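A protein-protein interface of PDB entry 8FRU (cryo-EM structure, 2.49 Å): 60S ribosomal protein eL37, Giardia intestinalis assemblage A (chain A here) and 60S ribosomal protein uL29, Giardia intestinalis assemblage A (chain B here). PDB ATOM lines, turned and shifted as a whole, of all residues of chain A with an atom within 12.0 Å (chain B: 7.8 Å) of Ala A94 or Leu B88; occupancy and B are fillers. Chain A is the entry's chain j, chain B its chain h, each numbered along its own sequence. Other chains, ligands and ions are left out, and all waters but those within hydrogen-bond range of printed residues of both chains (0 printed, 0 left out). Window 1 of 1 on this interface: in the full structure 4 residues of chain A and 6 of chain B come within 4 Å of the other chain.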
ATOM      1  N   HIS A  77      -9.144  21.983 -14.236  1.00  0.00           N
ATOM      2  CA  HIS A  77      -9.910  21.796 -15.460  1.00  0.00           C
ATOM      3  C   HIS A  77      -9.100  22.188 -16.689  1.00  0.00           C
ATOM      4  O   HIS A  77      -9.127  21.490 -17.711  1.00  0.00           O
ATOM      5  CB  HIS A  77     -11.209  22.596 -15.381  1.00  0.00           C
ATOM      6  CG  HIS A  77     -12.034  22.525 -16.625  1.00  0.00           C
ATOM      7  ND1 HIS A  77     -12.878  21.472 -16.896  1.00  0.00           N
ATOM      8  CD2 HIS A  77     -12.141  23.371 -17.673  1.00  0.00           C
ATOM      9  CE1 HIS A  77     -13.469  21.673 -18.059  1.00  0.00           C
ATOM     10  NE2 HIS A  77     -13.037  22.818 -18.551  1.00  0.00           N
ATOM     11  N   MET A  78      -8.384  23.309 -16.616  1.00  0.00           N
ATOM     12  CA  MET A  78      -7.588  23.749 -17.754  1.00  0.00           C
ATOM     13  C   MET A  78      -6.504  22.741 -18.089  1.00  0.00           C
ATOM     14  O   MET A  78      -6.263  22.449 -19.265  1.00  0.00           O
ATOM     15  CB  MET A  78      -6.975  25.116 -17.476  1.00  0.00           C
ATOM     16  CG  MET A  78      -7.911  26.273 -17.696  1.00  0.00           C
ATOM     17  SD  MET A  78      -7.028  27.767 -18.153  1.00  0.00           S
ATOM     18  CE  MET A  78      -8.346  28.951 -18.037  1.00  0.00           C
ATOM     19  N   LYS A  80      -6.577  19.506 -17.545  1.00  0.00           N
ATOM     20  CA  LYS A  80      -7.189  18.334 -18.160  1.00  0.00           C
ATOM     21  C   LYS A  80      -7.547  18.592 -19.617  1.00  0.00           C
ATOM     22  O   LYS A  80      -7.291  17.750 -20.487  1.00  0.00           O
ATOM     23  CB  LYS A  80      -8.426  17.919 -17.372  1.00  0.00           C
ATOM     24  CG  LYS A  80      -8.113  17.151 -16.111  1.00  0.00           C
ATOM     25  CD  LYS A  80      -9.363  16.547 -15.502  1.00  0.00           C
ATOM     26  CE  LYS A  80     -10.359  17.621 -15.097  1.00  0.00           C
ATOM     27  NZ  LYS A  80     -10.778  17.467 -13.676  1.00  0.00           N
ATOM     28  N   VAL A  81      -8.142  19.748 -19.908  1.00  0.00           N
ATOM     29  CA  VAL A  81      -8.555  20.025 -21.281  1.00  0.00           C
ATOM     30  C   VAL A  81      -7.343  20.193 -22.188  1.00  0.00           C
ATOM     31  O   VAL A  81      -7.340  19.723 -23.327  1.00  0.00           O
ATOM     32  CB  VAL A  81      -9.480  21.252 -21.340  1.00  0.00           C
ATOM     33  CG1 VAL A  81      -9.747  21.623 -22.782  1.00  0.00           C
ATOM     34  CG2 VAL A  81     -10.774  20.965 -20.637  1.00  0.00           C
ATOM     35  N   TYR A  82      -6.299  20.876 -21.715  1.00  0.00           N
ATOM     36  CA  TYR A  82      -5.110  21.039 -22.542  1.00  0.00           C
ATOM     37  C   TYR A  82      -4.467  19.697 -22.846  1.00  0.00           C
ATOM     38  O   TYR A  82      -4.009  19.462 -23.968  1.00  0.00           O
ATOM     39  CB  TYR A  82      -4.106  21.963 -21.863  1.00  0.00           C
ATOM     40  CG  TYR A  82      -4.429  23.431 -21.982  1.00  0.00           C
ATOM     41  CD1 TYR A  82      -5.719  23.899 -21.779  1.00  0.00           C
ATOM     42  CD2 TYR A  82      -3.438  24.355 -22.278  1.00  0.00           C
ATOM     43  CE1 TYR A  82      -6.014  25.242 -21.875  1.00  0.00           C
ATOM     44  CE2 TYR A  82      -3.724  25.702 -22.375  1.00  0.00           C
ATOM     45  CZ  TYR A  82      -5.012  26.138 -22.173  1.00  0.00           C
ATOM     46  OH  TYR A  82      -5.301  27.476 -22.271  1.00  0.00           O
ATOM     47  N   ALA A  84      -6.016  16.724 -22.949  1.00  0.00           N
ATOM     48  CA  ALA A  84      -6.872  15.975 -23.864  1.00  0.00           C
ATOM     49  C   ALA A  84      -6.777  16.480 -25.294  1.00  0.00           C
ATOM     50  O   ALA A  84      -7.114  15.743 -26.224  1.00  0.00           O
ATOM     51  CB  ALA A  84      -8.325  16.031 -23.405  1.00  0.00           C
ATOM     52  N   TYR A  85      -6.333  17.715 -25.492  1.00  0.00           N
ATOM     53  CA  TYR A  85      -6.255  18.329 -26.808  1.00  0.00           C
ATOM     54  C   TYR A  85      -4.921  18.052 -27.494  1.00  0.00           C
ATOM     55  O   TYR A  85      -4.889  17.619 -28.648  1.00  0.00           O
ATOM     56  CB  TYR A  85      -6.481  19.833 -26.673  1.00  0.00           C
ATOM     57  CG  TYR A  85      -6.582  20.579 -27.975  1.00  0.00           C
ATOM     58  CD1 TYR A  85      -5.447  21.042 -28.617  1.00  0.00           C
ATOM     59  CD2 TYR A  85      -7.811  20.842 -28.550  1.00  0.00           C
ATOM     60  CE1 TYR A  85      -5.535  21.727 -29.800  1.00  0.00           C
ATOM     61  CE2 TYR A  85      -7.906  21.529 -29.731  1.00  0.00           C
ATOM     62  CZ  TYR A  85      -6.766  21.969 -30.350  1.00  0.00           C
ATOM     63  OH  TYR A  85      -6.855  22.658 -31.530  1.00  0.00           O
ATOM     64  N   ASN A  86      -3.814  18.302 -26.795  1.00  0.00           N
ATOM     65  CA  ASN A  86      -2.499  18.151 -27.404  1.00  0.00           C
ATOM     66  C   ASN A  86      -2.190  16.695 -27.723  1.00  0.00           C
ATOM     67  O   ASN A  86      -1.583  16.397 -28.756  1.00  0.00           O
ATOM     68  CB  ASN A  86      -1.431  18.736 -26.486  1.00  0.00           C
ATOM     69  CG  ASN A  86      -1.458  20.247 -26.459  1.00  0.00           C
ATOM     70  OD1 ASN A  86      -1.858  20.853 -25.471  1.00  0.00           O
ATOM     71  ND2 ASN A  86      -1.032  20.864 -27.550  1.00  0.00           N
ATOM     72  N   GLY A  88      -4.532  13.358 -27.406  1.00  0.00           N
ATOM     73  CA  GLY A  88      -5.785  12.777 -26.980  1.00  0.00           C
ATOM     74  C   GLY A  88      -6.769  12.760 -28.128  1.00  0.00           C
ATOM     75  O   GLY A  88      -6.382  12.832 -29.294  1.00  0.00           O
ATOM     76  N   THR A  89      -8.049  12.678 -27.772  1.00  0.00           N
ATOM     77  CA  THR A  89      -9.109  12.456 -28.743  1.00  0.00           C
ATOM     78  C   THR A  89     -10.109  13.599 -28.812  1.00  0.00           C
ATOM     79  O   THR A  89     -11.196  13.422 -29.371  1.00  0.00           O
ATOM     80  CB  THR A  89      -9.836  11.153 -28.416  1.00  0.00           C
ATOM     81  OG1 THR A  89     -10.823  11.402 -27.408  1.00  0.00           O
ATOM     82  CG2 THR A  89      -8.852  10.130 -27.904  1.00  0.00           C
ATOM     83  N   LEU A  90      -9.783  14.762 -28.255  1.00  0.00           N
ATOM     84  CA  LEU A  90     -10.708  15.885 -28.327  1.00  0.00           C
ATOM     85  C   LEU A  90     -10.911  16.339 -29.767  1.00  0.00           C
ATOM     86  O   LEU A  90     -12.035  16.646 -30.176  1.00  0.00           O
ATOM     87  CB  LEU A  90     -10.198  17.031 -27.460  1.00  0.00           C
ATOM     88  CG  LEU A  90     -11.242  17.949 -26.838  1.00  0.00           C
ATOM     89  CD1 LEU A  90     -12.292  17.141 -26.101  1.00  0.00           C
ATOM     90  CD2 LEU A  90     -10.568  18.930 -25.907  1.00  0.00           C
ATOM     91  N   LYS A  91      -9.834  16.382 -30.555  1.00  0.00           N
ATOM     92  CA  LYS A  91      -9.948  16.825 -31.940  1.00  0.00           C
ATOM     93  C   LYS A  91     -10.728  15.830 -32.791  1.00  0.00           C
ATOM     94  O   LYS A  91     -11.541  16.228 -33.630  1.00  0.00           O
ATOM     95  CB  LYS A  91      -8.562  17.063 -32.532  1.00  0.00           C
ATOM     96  CG  LYS A  91      -8.072  18.483 -32.381  1.00  0.00           C
ATOM     97  CD  LYS A  91      -6.654  18.517 -31.864  1.00  0.00           C
ATOM     98  CE  LYS A  91      -5.693  19.030 -32.915  1.00  0.00           C
ATOM     99  NZ  LYS A  91      -4.285  18.803 -32.502  1.00  0.00           N
ATOM    100  N   ALA A  92     -10.489  14.532 -32.599  1.00  0.00           N
ATOM    101  CA  ALA A  92     -11.263  13.530 -33.324  1.00  0.00           C
ATOM    102  C   ALA A  92     -12.744  13.633 -32.988  1.00  0.00           C
ATOM    103  O   ALA A  92     -13.601  13.549 -33.875  1.00  0.00           O
ATOM    104  CB  ALA A  92     -10.739  12.132 -33.001  1.00  0.00           C
ATOM    105  N   ASN A  93     -13.058  13.816 -31.707  1.00  0.00           N
ATOM    106  CA  ASN A  93     -14.443  13.978 -31.292  1.00  0.00           C
ATOM    107  C   ASN A  93     -15.067  15.208 -31.933  1.00  0.00           C
ATOM    108  O   ASN A  93     -16.205  15.161 -32.410  1.00  0.00           O
ATOM    109  CB  ASN A  93     -14.513  14.078 -29.770  1.00  0.00           C
ATOM    110  CG  ASN A  93     -15.551  13.162 -29.174  1.00  0.00           C
ATOM    111  OD1 ASN A  93     -16.751  13.351 -29.375  1.00  0.00           O
ATOM    112  ND2 ASN A  93     -15.099  12.165 -28.431  1.00  0.00           N
ATOM    113  N   ALA A  94     -14.334  16.321 -31.951  1.00  0.00           N
ATOM    114  CA  ALA A  94     -14.856  17.535 -32.567  1.00  0.00           C
ATOM    115  C   ALA A  94     -15.104  17.333 -34.052  1.00  0.00           C
ATOM    116  O   ALA A  94     -16.119  17.789 -34.587  1.00  0.00           O
ATOM    117  CB  ALA A  94     -13.889  18.694 -32.340  1.00  0.00           C
ATOM    118  N   ARG A  95     -14.176  16.666 -34.738  1.00  0.00           N
ATOM    119  CA  ARG A  95     -14.334  16.432 -36.169  1.00  0.00           C
ATOM    120  C   ARG A  95     -15.548  15.564 -36.455  1.00  0.00           C
ATOM    121  O   ARG A  95     -16.306  15.833 -37.391  1.00  0.00           O
ATOM    122  CB  ARG A  95     -13.072  15.785 -36.729  1.00  0.00           C
ATOM    123  CG  ARG A  95     -12.415  16.568 -37.834  1.00  0.00           C
ATOM    124  CD  ARG A  95     -11.533  15.657 -38.645  1.00  0.00           C
ATOM    125  NE  ARG A  95     -10.992  14.580 -37.828  1.00  0.00           N
ATOM    126  CZ  ARG A  95      -9.842  14.642 -37.171  1.00  0.00           C
ATOM    127  NH1 ARG A  95      -9.085  15.726 -37.206  1.00  0.00           N
ATOM    128  NH2 ARG A  95      -9.442  13.591 -36.463  1.00  0.00           N
ATOM    129  N   LYS A  96     -15.745  14.512 -35.661  1.00  0.00           N
ATOM    130  CA  LYS A  96     -16.917  13.665 -35.848  1.00  0.00           C
ATOM    131  C   LYS A  96     -18.202  14.433 -35.570  1.00  0.00           C
ATOM    132  O   LYS A  96     -19.196  14.274 -36.286  1.00  0.00           O
ATOM    133  CB  LYS A  96     -16.824  12.432 -34.951  1.00  0.00           C
ATOM    134  CG  LYS A  96     -18.048  11.530 -35.010  1.00  0.00           C
ATOM    135  CD  LYS A  96     -18.683  11.360 -33.637  1.00  0.00           C
ATOM    136  CE  LYS A  96     -19.758  12.409 -33.381  1.00  0.00           C
ATOM    137  NZ  LYS A  96     -20.509  12.160 -32.117  1.00  0.00           N
ATOM    138  N   TYR A  97     -18.206  15.263 -34.529  1.00  0.00           N
ATOM    139  CA  TYR A  97     -19.413  16.005 -34.180  1.00  0.00           C
ATOM    140  C   TYR A  97     -19.760  17.037 -35.243  1.00  0.00           C
ATOM    141  O   TYR A  97     -20.939  17.251 -35.547  1.00  0.00           O
ATOM    142  CB  TYR A  97     -19.235  16.673 -32.819  1.00  0.00           C
ATOM    143  CG  TYR A  97     -20.405  17.523 -32.378  1.00  0.00           C
ATOM    144  CD1 TYR A  97     -20.484  18.868 -32.719  1.00  0.00           C
ATOM    145  CD2 TYR A  97     -21.428  16.979 -31.614  1.00  0.00           C
ATOM    146  CE1 TYR A  97     -21.551  19.642 -32.314  1.00  0.00           C
ATOM    147  CE2 TYR A  97     -22.497  17.746 -31.206  1.00  0.00           C
ATOM    148  CZ  TYR A  97     -22.556  19.073 -31.558  1.00  0.00           C
ATOM    149  OH  TYR A  97     -23.623  19.835 -31.146  1.00  0.00           O
ATOM    150  N   LEU A  98     -18.751  17.702 -35.806  1.00  0.00           N
ATOM    151  CA  LEU A  98     -19.022  18.715 -36.818  1.00  0.00           C
ATOM    152  C   LEU A  98     -19.408  18.079 -38.146  1.00  0.00           C
ATOM    153  O   LEU A  98     -20.355  18.529 -38.803  1.00  0.00           O
ATOM    154  CB  LEU A  98     -17.809  19.627 -36.979  1.00  0.00           C
ATOM    155  CG  LEU A  98     -17.459  20.441 -35.728  1.00  0.00           C
ATOM    156  CD1 LEU A  98     -16.157  21.215 -35.918  1.00  0.00           C
ATOM    157  CD2 LEU A  98     -18.596  21.379 -35.338  1.00  0.00           C
ATOM    158  N   ALA A  99     -18.706  17.028 -38.554  1.00  0.00           N
ATOM    159  CA  ALA A  99     -19.020  16.349 -39.803  1.00  0.00           C
ATOM    160  C   ALA A  99     -20.317  15.559 -39.679  1.00  0.00           C
ATOM    161  O   ALA A  99     -21.285  16.028 -39.082  1.00  0.00           O
ATOM    162  CB  ALA A  99     -17.887  15.439 -40.207  1.00  0.00           C
ATOM    163  N   ARG B  85     -24.353  14.289 -23.147  1.00  0.00           N
ATOM    164  CA  ARG B  85     -24.026  14.862 -24.436  1.00  0.00           C
ATOM    165  C   ARG B  85     -22.528  14.741 -24.706  1.00  0.00           C
ATOM    166  O   ARG B  85     -21.730  14.577 -23.784  1.00  0.00           O
ATOM    167  CB  ARG B  85     -24.466  16.319 -24.492  1.00  0.00           C
ATOM    168  CG  ARG B  85     -25.967  16.507 -24.551  1.00  0.00           C
ATOM    169  CD  ARG B  85     -26.361  17.834 -23.950  1.00  0.00           C
ATOM    170  NE  ARG B  85     -27.794  17.969 -23.738  1.00  0.00           N
ATOM    171  CZ  ARG B  85     -28.467  19.096 -23.905  1.00  0.00           C
ATOM    172  NH1 ARG B  85     -27.871  20.198 -24.320  1.00  0.00           N
ATOM    173  NH2 ARG B  85     -29.768  19.123 -23.634  1.00  0.00           N
ATOM    174  N   PRO B  86     -22.127  14.799 -25.974  1.00  0.00           N
ATOM    175  CA  PRO B  86     -20.719  14.564 -26.315  1.00  0.00           C
ATOM    176  C   PRO B  86     -19.791  15.584 -25.678  1.00  0.00           C
ATOM    177  O   PRO B  86     -20.140  16.749 -25.486  1.00  0.00           O
ATOM    178  CB  PRO B  86     -20.696  14.671 -27.843  1.00  0.00           C
ATOM    179  CG  PRO B  86     -22.093  14.555 -28.279  1.00  0.00           C
ATOM    180  CD  PRO B  86     -22.980  14.954 -27.160  1.00  0.00           C
ATOM    181  N   LYS B  87     -18.586  15.127 -25.357  1.00  0.00           N
ATOM    182  CA  LYS B  87     -17.606  15.956 -24.669  1.00  0.00           C
ATOM    183  C   LYS B  87     -16.897  16.865 -25.667  1.00  0.00           C
ATOM    184  O   LYS B  87     -16.183  16.388 -26.552  1.00  0.00           O
ATOM    185  CB  LYS B  87     -16.603  15.076 -23.932  1.00  0.00           C
ATOM    186  CG  LYS B  87     -15.638  15.839 -23.057  1.00  0.00           C
ATOM    187  CD  LYS B  87     -14.854  14.896 -22.173  1.00  0.00           C
ATOM    188  CE  LYS B  87     -14.073  13.896 -23.003  1.00  0.00           C
ATOM    189  NZ  LYS B  87     -12.641  13.835 -22.594  1.00  0.00           N
ATOM    190  N   LEU B  88     -17.094  18.172 -25.519  1.00  0.00           N
ATOM    191  CA  LEU B  88     -16.463  19.176 -26.358  1.00  0.00           C
ATOM    192  C   LEU B  88     -16.113  20.370 -25.482  1.00  0.00           C
ATOM    193  O   LEU B  88     -16.398  20.385 -24.284  1.00  0.00           O
ATOM    194  CB  LEU B  88     -17.380  19.588 -27.513  1.00  0.00           C
ATOM    195  CG  LEU B  88     -17.849  18.503 -28.482  1.00  0.00           C
ATOM    196  CD1 LEU B  88     -19.123  18.928 -29.170  1.00  0.00           C
ATOM    197  CD2 LEU B  88     -16.772  18.207 -29.499  1.00  0.00           C
ATOM    198  N   THR B  89     -15.492  21.379 -26.075  1.00  0.00           N
ATOM    199  CA  THR B  89     -15.306  22.632 -25.364  1.00  0.00           C
ATOM    200  C   THR B  89     -16.466  23.578 -25.655  1.00  0.00           C
ATOM    201  O   THR B  89     -17.258  23.374 -26.572  1.00  0.00           O
ATOM    202  CB  THR B  89     -13.974  23.295 -25.736  1.00  0.00           C
ATOM    203  OG1 THR B  89     -13.964  23.630 -27.125  1.00  0.00           O
ATOM    204  CG2 THR B  89     -12.811  22.382 -25.431  1.00  0.00           C
ATOM    205  N   HIS B  90     -16.564  24.618 -24.836  1.00  0.00           N
ATOM    206  CA  HIS B  90     -17.569  25.653 -25.035  1.00  0.00           C
ATOM    207  C   HIS B  90     -17.478  26.238 -26.442  1.00  0.00           C
ATOM    208  O   HIS B  90     -18.485  26.361 -27.153  1.00  0.00           O
ATOM    209  CB  HIS B  90     -17.362  26.720 -23.957  1.00  0.00           C
ATOM    210  CG  HIS B  90     -18.401  27.793 -23.926  1.00  0.00           C
ATOM    211  ND1 HIS B  90     -19.191  28.021 -22.823  1.00  0.00           N
ATOM    212  CD2 HIS B  90     -18.745  28.732 -24.834  1.00  0.00           C
ATOM    213  CE1 HIS B  90     -19.997  29.037 -23.064  1.00  0.00           C
ATOM    214  NE2 HIS B  90     -19.746  29.486 -24.278  1.00  0.00           N
ATOM    215  N   ALA B  91     -16.260  26.570 -26.871  1.00  0.00           N
ATOM    216  CA  ALA B  91     -16.070  27.252 -28.144  1.00  0.00           C
ATOM    217  C   ALA B  91     -16.433  26.363 -29.324  1.00  0.00           C
ATOM    218  O   ALA B  91     -17.056  26.826 -30.283  1.00  0.00           O
ATOM    219  CB  ALA B  91     -14.631  27.738 -28.264  1.00  0.00           C
ATOM    220  N   MET B  92     -16.039  25.091 -29.292  1.00  0.00           N
ATOM    221  CA  MET B  92     -16.411  24.209 -30.386  1.00  0.00           C
ATOM    222  C   MET B  92     -17.856  23.752 -30.297  1.00  0.00           C
ATOM    223  O   MET B  92     -18.420  23.333 -31.309  1.00  0.00           O
ATOM    224  CB  MET B  92     -15.481  22.997 -30.450  1.00  0.00           C
ATOM    225  CG  MET B  92     -15.663  21.990 -29.353  1.00  0.00           C
ATOM    226  SD  MET B  92     -14.330  20.777 -29.328  1.00  0.00           S
ATOM    227  CE  MET B  92     -12.943  21.765 -29.866  1.00  0.00           C
ATOM    228  N   ARG B  93     -18.471  23.824 -29.119  1.00  0.00           N
ATOM    229  CA  ARG B  93     -19.908  23.595 -29.037  1.00  0.00           C
ATOM    230  C   ARG B  93     -20.675  24.696 -29.752  1.00  0.00           C
ATOM    231  O   ARG B  93     -21.667  24.423 -30.435  1.00  0.00           O
ATOM    232  CB  ARG B  93     -20.351  23.499 -27.582  1.00  0.00           C
ATOM    233  CG  ARG B  93     -20.949  22.167 -27.213  1.00  0.00           C
ATOM    234  CD  ARG B  93     -20.723  21.854 -25.758  1.00  0.00           C
ATOM    235  NE  ARG B  93     -21.190  22.932 -24.900  1.00  0.00           N
ATOM    236  CZ  ARG B  93     -20.662  23.230 -23.722  1.00  0.00           C
ATOM    237  NH1 ARG B  93     -19.654  22.537 -23.223  1.00  0.00           N
ATOM    238  NH2 ARG B  93     -21.155  24.252 -23.033  1.00  0.00           N
ATOM    239  N   CYS B  94     -20.237  25.942 -29.610  1.00  0.00           N
ATOM    240  CA  CYS B  94     -20.975  27.056 -30.211  1.00  0.00           C
ATOM    241  C   CYS B  94     -20.488  27.397 -31.620  1.00  0.00           C
ATOM    242  O   CYS B  94     -20.211  28.554 -31.916  1.00  0.00           O
ATOM    243  CB  CYS B  94     -20.886  28.273 -29.301  1.00  0.00           C
ATOM    244  SG  CYS B  94     -21.696  28.078 -27.700  1.00  0.00           S
ATOM    245  N   GLN B  95     -20.419  26.415 -32.519  1.00  0.00           N
ATOM    246  CA  GLN B  95     -19.774  26.610 -33.812  1.00  0.00           C
ATOM    247  C   GLN B  95     -20.590  25.996 -34.940  1.00  0.00           C
ATOM    248  O   GLN B  95     -21.357  25.053 -34.731  1.00  0.00           O
ATOM    249  CB  GLN B  95     -18.380  25.999 -33.823  1.00  0.00           C
ATOM    250  CG  GLN B  95     -17.305  26.963 -34.207  1.00  0.00           C
ATOM    251  CD  GLN B  95     -15.935  26.420 -33.919  1.00  0.00           C
ATOM    252  OE1 GLN B  95     -15.673  25.234 -34.115  1.00  0.00           O
ATOM    253  NE2 GLN B  95     -15.052  27.281 -33.431  1.00  0.00           N
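Ala A94 touches just these residues of chain B: Leu B88 (3.7 Å) and Met B92 (3.7 Å). Leu B88 touches just these residues of chain A: Ala A94 (3.7 Å) and Tyr A97 (3.7 Å). Pro B86 touches none of the printed residues of chain A. No residue of chain A comes within 4 Å of Thr B89. Of chain A, only Ala A94 (3.7 Å) comes within 4 Å of Met B92. Arg B93 touches none of the printed residues of chain A. Of the printed residues of chain B, Leu A90 touches Lys B87. Of the printed residues of chain A, Lys B87 touches Leu A90. Val A81 touches none of the printed residues of chain B. His B90 touches none of the printed residues of chain A. The nearest residue of chain A that does not touch Leu B88 is Asn A93 (4.2 Å).
Among the printed residues, pairs that only touch across the chains: Ala A94 with Leu B88 (3.7 Å), Ala A94 with Met B92 (3.7 Å), Tyr A97 with Leu B88 (3.7 Å) and Leu A90 with Lys B87 (3.99 Å).
Hydrophobic or aromatic side chains of chain A within 4 Å of the printed part of chain B: Leu A90, Ala A94 and Tyr A97. Of the 11 printed residues of chain B, 3 touch a printed residue of chain A. Hydrophobic or aromatic side chains of chain B that line the printed part of chain A: Leu B88 and Met B92. Among the printed residues, 4 pairs touch across the chains. Among the printed residues, no Asp or Glu carboxylate lies within 4 Å of a Lys or Arg side-chain nitrogen of the other chain.
The side-chain hydroxyl (OG1) of Thr B89 sits close to the backbone NH (N) of Met B92 (3.3 Å). The backbone carbonyl oxygen (O) of Ala A84 lies within hydrogen-bond range of the backbone NH (N) of Leu A90, 3.5 Å away.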
